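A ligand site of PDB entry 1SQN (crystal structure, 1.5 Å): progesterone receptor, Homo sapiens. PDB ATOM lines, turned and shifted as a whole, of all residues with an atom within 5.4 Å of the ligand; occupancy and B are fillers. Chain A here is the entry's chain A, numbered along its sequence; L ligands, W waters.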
ATOM      1  N   LEU A  43      11.595 -15.311   4.284  1.00  0.00           N
ATOM      2  CA  LEU A  43      11.087 -14.133   5.032  1.00  0.00           C
ATOM      3  C   LEU A  43      10.765 -12.959   4.106  1.00  0.00           C
ATOM      4  O   LEU A  43       9.710 -12.282   4.280  1.00  0.00           O
ATOM      5  CB  LEU A  43      12.127 -13.768   6.032  1.00  0.00           C
ATOM      6  CG  LEU A  43      12.255 -14.805   7.164  1.00  0.00           C
ATOM      7  CD1 LEU A  43      13.422 -14.469   8.087  1.00  0.00           C
ATOM      8  CD2 LEU A  43      11.026 -14.869   7.960  1.00  0.00           C
ATOM      9  N   LEU A  46       7.558 -13.761   2.305  1.00  0.00           N
ATOM     10  CA  LEU A  46       6.427 -13.596   3.219  1.00  0.00           C
ATOM     11  C   LEU A  46       6.106 -12.073   3.417  1.00  0.00           C
ATOM     12  O   LEU A  46       4.874 -11.704   3.517  1.00  0.00           O
ATOM     13  CB  LEU A  46       6.716 -14.221   4.545  1.00  0.00           C
ATOM     14  CG  LEU A  46       6.726 -15.763   4.525  1.00  0.00           C
ATOM     15  CD1 LEU A  46       7.332 -16.280   5.830  1.00  0.00           C
ATOM     16  CD2 LEU A  46       5.197 -16.193   4.460  1.00  0.00           C
ATOM     17  N   ASN A  47       7.130 -11.252   3.497  1.00  0.00           N
ATOM     18  CA  ASN A  47       6.873  -9.792   3.613  1.00  0.00           C
ATOM     19  C   ASN A  47       6.291  -9.196   2.363  1.00  0.00           C
ATOM     20  O   ASN A  47       5.440  -8.291   2.437  1.00  0.00           O
ATOM     21  CB  ASN A  47       8.152  -9.017   3.975  1.00  0.00           C
ATOM     22  CG  ASN A  47       8.681  -9.405   5.353  1.00  0.00           C
ATOM     23  OD1 ASN A  47       7.962  -9.918   6.226  1.00  0.00           O
ATOM     24  ND2 ASN A  47       9.987  -9.111   5.594  1.00  0.00           N
ATOM     25  N   LEU A  49       4.348 -10.852   0.287  1.00  0.00           N
ATOM     26  CA  LEU A  49       2.947 -11.281   0.330  1.00  0.00           C
ATOM     27  C   LEU A  49       2.184 -10.404   1.325  1.00  0.00           C
ATOM     28  O   LEU A  49       1.046  -9.976   1.064  1.00  0.00           O
ATOM     29  CB  LEU A  49       2.920 -12.712   0.860  1.00  0.00           C
ATOM     30  CG  LEU A  49       1.512 -13.233   0.895  1.00  0.00           C
ATOM     31  CD1 LEU A  49       0.837 -13.223  -0.540  1.00  0.00           C
ATOM     32  CD2 LEU A  49       1.627 -14.870   1.409  1.00  0.00           C
ATOM     33  N   GLY A  50       2.815 -10.046   2.408  1.00  0.00           N
ATOM     34  CA  GLY A  50       2.235  -9.184   3.485  1.00  0.00           C
ATOM     35  C   GLY A  50       1.880  -7.818   2.880  1.00  0.00           C
ATOM     36  O   GLY A  50       0.778  -7.270   3.124  1.00  0.00           O
ATOM     37  N   GLN A  53      -1.182  -8.209   0.745  1.00  0.00           N
ATOM     38  CA  GLN A  53      -2.375  -8.430   1.509  1.00  0.00           C
ATOM     39  C   GLN A  53      -2.831  -7.184   2.258  1.00  0.00           C
ATOM     40  O   GLN A  53      -4.019  -6.948   2.451  1.00  0.00           O
ATOM     41  CB  GLN A  53      -2.178  -9.598   2.497  1.00  0.00           C
ATOM     42  CG  GLN A  53      -2.023 -10.925   1.795  1.00  0.00           C
ATOM     43  CD  GLN A  53      -2.063 -12.081   2.730  1.00  0.00           C
ATOM     44  OE1 GLN A  53      -2.017 -13.291   2.281  1.00  0.00           O
ATOM     45  NE2 GLN A  53      -2.278 -11.830   4.014  1.00  0.00           N
ATOM     46  N   TRP A  83      -4.035  -5.565  11.397  1.00  0.00           N
ATOM     47  CA  TRP A  83      -3.522  -6.208  10.177  1.00  0.00           C
ATOM     48  C   TRP A  83      -2.914  -7.580  10.421  1.00  0.00           C
ATOM     49  O   TRP A  83      -3.172  -8.527   9.624  1.00  0.00           O
ATOM     50  CB  TRP A  83      -2.582  -5.323   9.433  1.00  0.00           C
ATOM     51  CG  TRP A  83      -1.307  -5.125  10.073  1.00  0.00           C
ATOM     52  CD1 TRP A  83      -0.970  -4.072  10.946  1.00  0.00           C
ATOM     53  CD2 TRP A  83      -0.077  -5.863   9.849  1.00  0.00           C
ATOM     54  NE1 TRP A  83       0.346  -4.229  11.368  1.00  0.00           N
ATOM     55  CE2 TRP A  83       0.897  -5.280  10.686  1.00  0.00           C
ATOM     56  CE3 TRP A  83       0.250  -7.019   9.144  1.00  0.00           C
ATOM     57  CZ2 TRP A  83       2.199  -5.781  10.803  1.00  0.00           C
ATOM     58  CZ3 TRP A  83       1.577  -7.517   9.262  1.00  0.00           C
ATOM     59  CH2 TRP A  83       2.522  -6.856  10.058  1.00  0.00           C
ATOM     60  N   MET A  84      -2.080  -7.739  11.431  1.00  0.00           N
ATOM     61  CA  MET A  84      -1.455  -9.066  11.642  1.00  0.00           C
ATOM     62  C   MET A  84      -2.553 -10.105  11.962  1.00  0.00           C
ATOM     63  O   MET A  84      -2.483 -11.281  11.507  1.00  0.00           O
ATOM     64  CB  MET A  84      -0.407  -8.975  12.801  1.00  0.00           C
ATOM     65  CG  MET A  84       0.281 -10.304  13.111  1.00  0.00           C
ATOM     66  SD  MET A  84       1.565 -10.497  11.859  1.00  0.00           S
ATOM     67  CE  MET A  84       2.728  -9.229  12.490  1.00  0.00           C
ATOM     68  N   MET A  87      -4.309 -11.088   8.844  1.00  0.00           N
ATOM     69  CA  MET A  87      -3.463 -11.908   7.981  1.00  0.00           C
ATOM     70  C   MET A  87      -3.368 -13.354   8.472  1.00  0.00           C
ATOM     71  O   MET A  87      -3.514 -14.280   7.670  1.00  0.00           O
ATOM     72  CB  MET A  87      -2.075 -11.286   7.793  1.00  0.00           C
ATOM     73  CG  MET A  87      -2.167 -10.016   6.917  1.00  0.00           C
ATOM     74  SD  MET A  87      -0.487  -9.498   6.486  1.00  0.00           S
ATOM     75  CE  MET A  87      -0.905  -7.906   5.694  1.00  0.00           C
ATOM     76  N   VAL A  88      -3.122 -13.532   9.760  1.00  0.00           N
ATOM     77  CA  VAL A  88      -3.045 -14.919  10.288  1.00  0.00           C
ATOM     78  C   VAL A  88      -4.382 -15.607  10.288  1.00  0.00           C
ATOM     79  O   VAL A  88      -4.404 -16.828  10.067  1.00  0.00           O
ATOM     80  CB  VAL A  88      -2.355 -14.946  11.665  1.00  0.00           C
ATOM     81  CG1 VAL A  88      -3.282 -14.381  12.774  1.00  0.00           C
ATOM     82  CG2 VAL A  88      -1.810 -16.366  12.046  1.00  0.00           C
ATOM     83  N   LEU A  91      -4.865 -16.735   6.775  1.00  0.00           N
ATOM     84  CA  LEU A  91      -3.950 -17.875   6.539  1.00  0.00           C
ATOM     85  C   LEU A  91      -4.629 -19.092   7.079  1.00  0.00           C
ATOM     86  O   LEU A  91      -4.601 -20.183   6.439  1.00  0.00           O
ATOM     87  CB  LEU A  91      -2.600 -17.653   7.246  1.00  0.00           C
ATOM     88  CG  LEU A  91      -1.747 -18.876   7.471  1.00  0.00           C
ATOM     89  CD1 LEU A  91      -1.296 -19.320   6.137  1.00  0.00           C
ATOM     90  CD2 LEU A  91      -0.557 -18.465   8.345  1.00  0.00           C
ATOM     91  N   ARG A  94      -7.484 -20.231   4.668  1.00  0.00           N
ATOM     92  CA  ARG A  94      -6.965 -20.856   3.425  1.00  0.00           C
ATOM     93  C   ARG A  94      -6.306 -22.241   3.697  1.00  0.00           C
ATOM     94  O   ARG A  94      -6.465 -23.185   2.869  1.00  0.00           O
ATOM     95  CB  ARG A  94      -5.987 -20.033   2.689  1.00  0.00           C
ATOM     96  CG  ARG A  94      -6.550 -18.600   2.263  1.00  0.00           C
ATOM     97  CD  ARG A  94      -5.463 -17.898   1.378  1.00  0.00           C
ATOM     98  NE  ARG A  94      -4.289 -17.553   2.099  1.00  0.00           N
ATOM     99  CZ  ARG A  94      -4.202 -16.537   2.922  1.00  0.00           C
ATOM    100  NH1 ARG A  94      -3.069 -16.247   3.565  1.00  0.00           N
ATOM    101  NH2 ARG A  94      -5.249 -15.728   3.099  1.00  0.00           N
ATOM    102  N   PHE A 106      -0.038 -20.001   2.757  1.00  0.00           N
ATOM    103  CA  PHE A 106       0.137 -18.536   2.679  1.00  0.00           C
ATOM    104  C   PHE A 106      -0.431 -17.948   1.358  1.00  0.00           C
ATOM    105  O   PHE A 106      -1.121 -16.905   1.327  1.00  0.00           O
ATOM    106  CB  PHE A 106       1.607 -18.179   2.819  1.00  0.00           C
ATOM    107  CG  PHE A 106       2.119 -18.394   4.223  1.00  0.00           C
ATOM    108  CD1 PHE A 106       2.654 -19.670   4.538  1.00  0.00           C
ATOM    109  CD2 PHE A 106       1.979 -17.444   5.174  1.00  0.00           C
ATOM    110  CE1 PHE A 106       3.181 -19.905   5.841  1.00  0.00           C
ATOM    111  CE2 PHE A 106       2.522 -17.671   6.517  1.00  0.00           C
ATOM    112  CZ  PHE A 106       3.105 -18.907   6.848  1.00  0.00           C
ATOM    113  N   PHE A 122      11.385 -20.004  13.471  1.00  0.00           N
ATOM    114  CA  PHE A 122      10.352 -19.864  12.434  1.00  0.00           C
ATOM    115  C   PHE A 122       9.401 -21.060  12.540  1.00  0.00           C
ATOM    116  O   PHE A 122       8.205 -20.932  12.399  1.00  0.00           O
ATOM    117  CB  PHE A 122      10.955 -19.783  11.019  1.00  0.00           C
ATOM    118  CG  PHE A 122       9.935 -19.650   9.911  1.00  0.00           C
ATOM    119  CD1 PHE A 122       9.013 -18.575   9.873  1.00  0.00           C
ATOM    120  CD2 PHE A 122       9.824 -20.636   8.933  1.00  0.00           C
ATOM    121  CE1 PHE A 122       8.096 -18.463   8.910  1.00  0.00           C
ATOM    122  CE2 PHE A 122       8.853 -20.551   7.971  1.00  0.00           C
ATOM    123  CZ  PHE A 122       7.979 -19.436   7.949  1.00  0.00           C
ATOM    124  N   LEU A 125       7.184 -20.367  15.419  1.00  0.00           N
ATOM    125  CA  LEU A 125       6.161 -19.387  14.986  1.00  0.00           C
ATOM    126  C   LEU A 125       5.051 -20.077  14.159  1.00  0.00           C
ATOM    127  O   LEU A 125       3.902 -19.771  14.313  1.00  0.00           O
ATOM    128  CB  LEU A 125       6.842 -18.378  14.046  1.00  0.00           C
ATOM    129  CG  LEU A 125       5.891 -17.300  13.505  1.00  0.00           C
ATOM    130  CD1 LEU A 125       5.515 -16.339  14.597  1.00  0.00           C
ATOM    131  CD2 LEU A 125       6.554 -16.579  12.316  1.00  0.00           C
ATOM    132  N   MET A 129       0.958 -20.285  14.649  1.00  0.00           N
ATOM    133  CA  MET A 129      -0.063 -19.951  13.615  1.00  0.00           C
ATOM    134  C   MET A 129      -0.945 -21.116  13.286  1.00  0.00           C
ATOM    135  O   MET A 129      -2.125 -20.927  12.993  1.00  0.00           O
ATOM    136  CB  MET A 129       0.627 -19.439  12.366  1.00  0.00           C
ATOM    137  CG  MET A 129       1.436 -18.153  12.648  1.00  0.00           C
ATOM    138  SD  MET A 129       2.009 -17.326  11.223  1.00  0.00           S
ATOM    139  CE  MET A 129       3.180 -18.328  10.602  1.00  0.00           C
ATOM    140  N   LEU A 215       3.384 -13.185  17.097  1.00  0.00           N
ATOM    141  CA  LEU A 215       3.688 -12.799  15.749  1.00  0.00           C
ATOM    142  C   LEU A 215       4.195 -11.342  15.701  1.00  0.00           C
ATOM    143  O   LEU A 215       5.115 -10.983  14.923  1.00  0.00           O
ATOM    144  CB  LEU A 215       2.431 -12.837  14.872  1.00  0.00           C
ATOM    145  CG  LEU A 215       2.013 -14.202  14.369  1.00  0.00           C
ATOM    146  CD1 LEU A 215       1.898 -15.299  15.449  1.00  0.00           C
ATOM    147  CD2 LEU A 215       0.701 -14.072  13.649  1.00  0.00           C
ATOM    148  N   TYR A 218       7.825 -11.397  16.866  1.00  0.00           N
ATOM    149  CA  TYR A 218       8.720 -11.917  15.857  1.00  0.00           C
ATOM    150  C   TYR A 218       8.913 -10.927  14.735  1.00  0.00           C
ATOM    151  O   TYR A 218       9.993 -10.696  14.162  1.00  0.00           O
ATOM    152  CB  TYR A 218       8.122 -13.263  15.352  1.00  0.00           C
ATOM    153  CG  TYR A 218       9.042 -14.053  14.475  1.00  0.00           C
ATOM    154  CD1 TYR A 218       9.296 -13.682  13.149  1.00  0.00           C
ATOM    155  CD2 TYR A 218       9.684 -15.212  14.990  1.00  0.00           C
ATOM    156  CE1 TYR A 218      10.157 -14.440  12.373  1.00  0.00           C
ATOM    157  CE2 TYR A 218      10.522 -15.976  14.169  1.00  0.00           C
ATOM    158  CZ  TYR A 218      10.747 -15.586  12.882  1.00  0.00           C
ATOM    159  OH  TYR A 218      11.624 -16.338  12.101  1.00  0.00           O
ATOM    160  N   CYS A 219       7.808 -10.333  14.255  1.00  0.00           N
ATOM    161  CA  CYS A 219       7.949  -9.379  13.148  1.00  0.00           C
ATOM    162  C   CYS A 219       8.793  -8.162  13.505  1.00  0.00           C
ATOM    163  O   CYS A 219       9.658  -7.768  12.716  1.00  0.00           O
ATOM    164  CB  CYS A 219       6.512  -8.946  12.795  1.00  0.00           C
ATOM    165  SG  CYS A 219       6.392  -7.604  11.575  1.00  0.00           S
ATOM    166  N   THR A 222      12.397  -9.120  13.550  1.00  0.00           N
ATOM    167  CA  THR A 222      12.907  -9.351  12.227  1.00  0.00           C
ATOM    168  C   THR A 222      13.112  -8.001  11.506  1.00  0.00           C
ATOM    169  O   THR A 222      14.092  -7.825  10.748  1.00  0.00           O
ATOM    170  CB  THR A 222      11.948 -10.301  11.411  1.00  0.00           C
ATOM    171  OG1 THR A 222      11.841 -11.534  12.113  1.00  0.00           O
ATOM    172  CG2 THR A 222      12.550 -10.550  10.036  1.00  0.00           C
ATOM    173  N   PHE A 233      11.700  -5.526   3.748  1.00  0.00           N
ATOM    174  CA  PHE A 233      10.347  -5.181   4.144  1.00  0.00           C
ATOM    175  C   PHE A 233       9.872  -4.055   3.264  1.00  0.00           C
ATOM    176  O   PHE A 233      10.481  -2.949   3.209  1.00  0.00           O
ATOM    177  CB  PHE A 233      10.282  -4.663   5.576  1.00  0.00           C
ATOM    178  CG  PHE A 233      10.372  -5.723   6.659  1.00  0.00           C
ATOM    179  CD1 PHE A 233      11.591  -6.252   7.002  1.00  0.00           C
ATOM    180  CD2 PHE A 233       9.215  -6.213   7.254  1.00  0.00           C
ATOM    181  CE1 PHE A 233      11.658  -7.239   7.969  1.00  0.00           C
ATOM    182  CE2 PHE A 233       9.237  -7.229   8.205  1.00  0.00           C
ATOM    183  CZ  PHE A 233      10.455  -7.745   8.601  1.00  0.00           C
ATOM    184  N   MET A 237       4.135  -2.073   4.505  1.00  0.00           N
ATOM    185  CA  MET A 237       4.295  -2.938   5.722  1.00  0.00           C
ATOM    186  C   MET A 237       5.247  -2.299   6.730  1.00  0.00           C
ATOM    187  O   MET A 237       4.990  -2.259   7.930  1.00  0.00           O
ATOM    188  CB  MET A 237       4.884  -4.300   5.276  1.00  0.00           C
ATOM    189  CG  MET A 237       5.105  -5.210   6.532  1.00  0.00           C
ATOM    190  SD  MET A 237       5.342  -6.896   5.769  1.00  0.00           S
ATOM    191  CE  MET A 237       5.286  -7.889   7.152  1.00  0.00           C
HETATM  192  O1  LIG L   1      -0.921 -14.830   4.554  1.00  0.00           O
HETATM  193  C1  LIG L   1      -0.177 -14.149   5.235  1.00  0.00           C
HETATM  194  C2  LIG L   1       0.697 -13.053   4.600  1.00  0.00           C
HETATM  195  C3  LIG L   1      -0.084 -14.466   6.632  1.00  0.00           C
HETATM  196  C4  LIG L   1       0.883 -13.759   7.430  1.00  0.00           C
HETATM  197  C5  LIG L   1       0.768 -14.002   8.925  1.00  0.00           C
HETATM  198  C6  LIG L   1       1.886 -12.912   6.895  1.00  0.00           C
HETATM  199  C7  LIG L   1       2.000 -13.064   5.373  1.00  0.00           C
HETATM  200  C8  LIG L   1       3.128 -12.905   7.679  1.00  0.00           C
HETATM  201  C9  LIG L   1       3.141 -13.096   9.069  1.00  0.00           C
HETATM  202  C10 LIG L   1       2.124 -14.152   9.512  1.00  0.00           C
HETATM  203  C11 LIG L   1       4.235 -12.006   7.107  1.00  0.00           C
HETATM  204  C12 LIG L   1       5.582 -12.066   7.967  1.00  0.00           C
HETATM  205  C13 LIG L   1       5.404 -12.033   9.446  1.00  0.00           C
HETATM  206  C14 LIG L   1       4.344 -13.047   9.860  1.00  0.00           C
HETATM  207  C15 LIG L   1       4.947 -10.592   9.728  1.00  0.00           C
HETATM  208  C16 LIG L   1       6.615 -12.396  10.353  1.00  0.00           C
HETATM  209  O2  LIG L   1       7.592 -11.370  10.529  1.00  0.00           O
HETATM  210  C17 LIG L   1       5.918 -12.724  11.700  1.00  0.00           C
HETATM  211  C18 LIG L   1       4.511 -13.224  11.358  1.00  0.00           C
HETATM  212  C19 LIG L   1       7.353 -13.563   9.831  1.00  0.00           C
HETATM  213  C20 LIG L   1       7.977 -14.553   9.320  1.00  0.00           C
HETATM  214  O   HOH W   1       9.230 -11.370   8.285  1.00  0.00           O
HETATM  215  O   HOH W   2      -3.910 -13.762   5.099  1.00  0.00           O
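An oxygen (O1) of the ligand sits at hydrogen-bond distance from the guanidinium group of Arg 94 (2.8 Å). O1 of the ligand sits close to OE1 of Gln 53, at 3.0 Å.
OE1 of Gln 53 is in hydrogen-bond range of NH1 of Arg 94. The side-chain amide nitrogen (ND2) of Asn 47 sits close to the backbone carbonyl oxygen (O) of Leu 43 (3.4 Å). O of Tyr 218 lies within hydrogen-bond range of OG1 of Thr 222 (2.9 Å). NH1 of Arg 94 sits at hydrogen-bond distance from O of Phe 106 (3.0 Å).
Merely in contact with the ligand: Leu 43 (3.4 Å), Leu 46 (3.7 Å), Asn 47 (3.6 Å), Leu 49 (3.8 Å), Met 84 (3.8 Å), Met 87 (3.6 Å), Phe 106 (3.8 Å), Phe 122 (3.9 Å), Leu 125 (3.9 Å), Met 129 (3.6 Å), Leu 215 (3.8 Å), Tyr 218 (3.8 Å), Cys 219 (3.3 Å) and Met 237 (3.7 Å). 16 residues have an atom within 4 Å of the ligand: Leu 43, Leu 46, Asn 47, Leu 49, Gln 53, Met 84, Met 87, Arg 94, Phe 106, Phe 122, Leu 125, Met 129, Leu 215, Tyr 218, Cys 219 and Met 237.
Water W1 bridges O2 of the ligand (2.8 Å) and OD1 of Asn 47 (2.8 Å). Water W2 lies within hydrogen-bond range of O of Met 87 (2.7 Å), NE2 of Gln 53 (2.8 Å), NH1 of Arg 94 (3.0 Å) and O1 of the ligand (3.2 Å).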
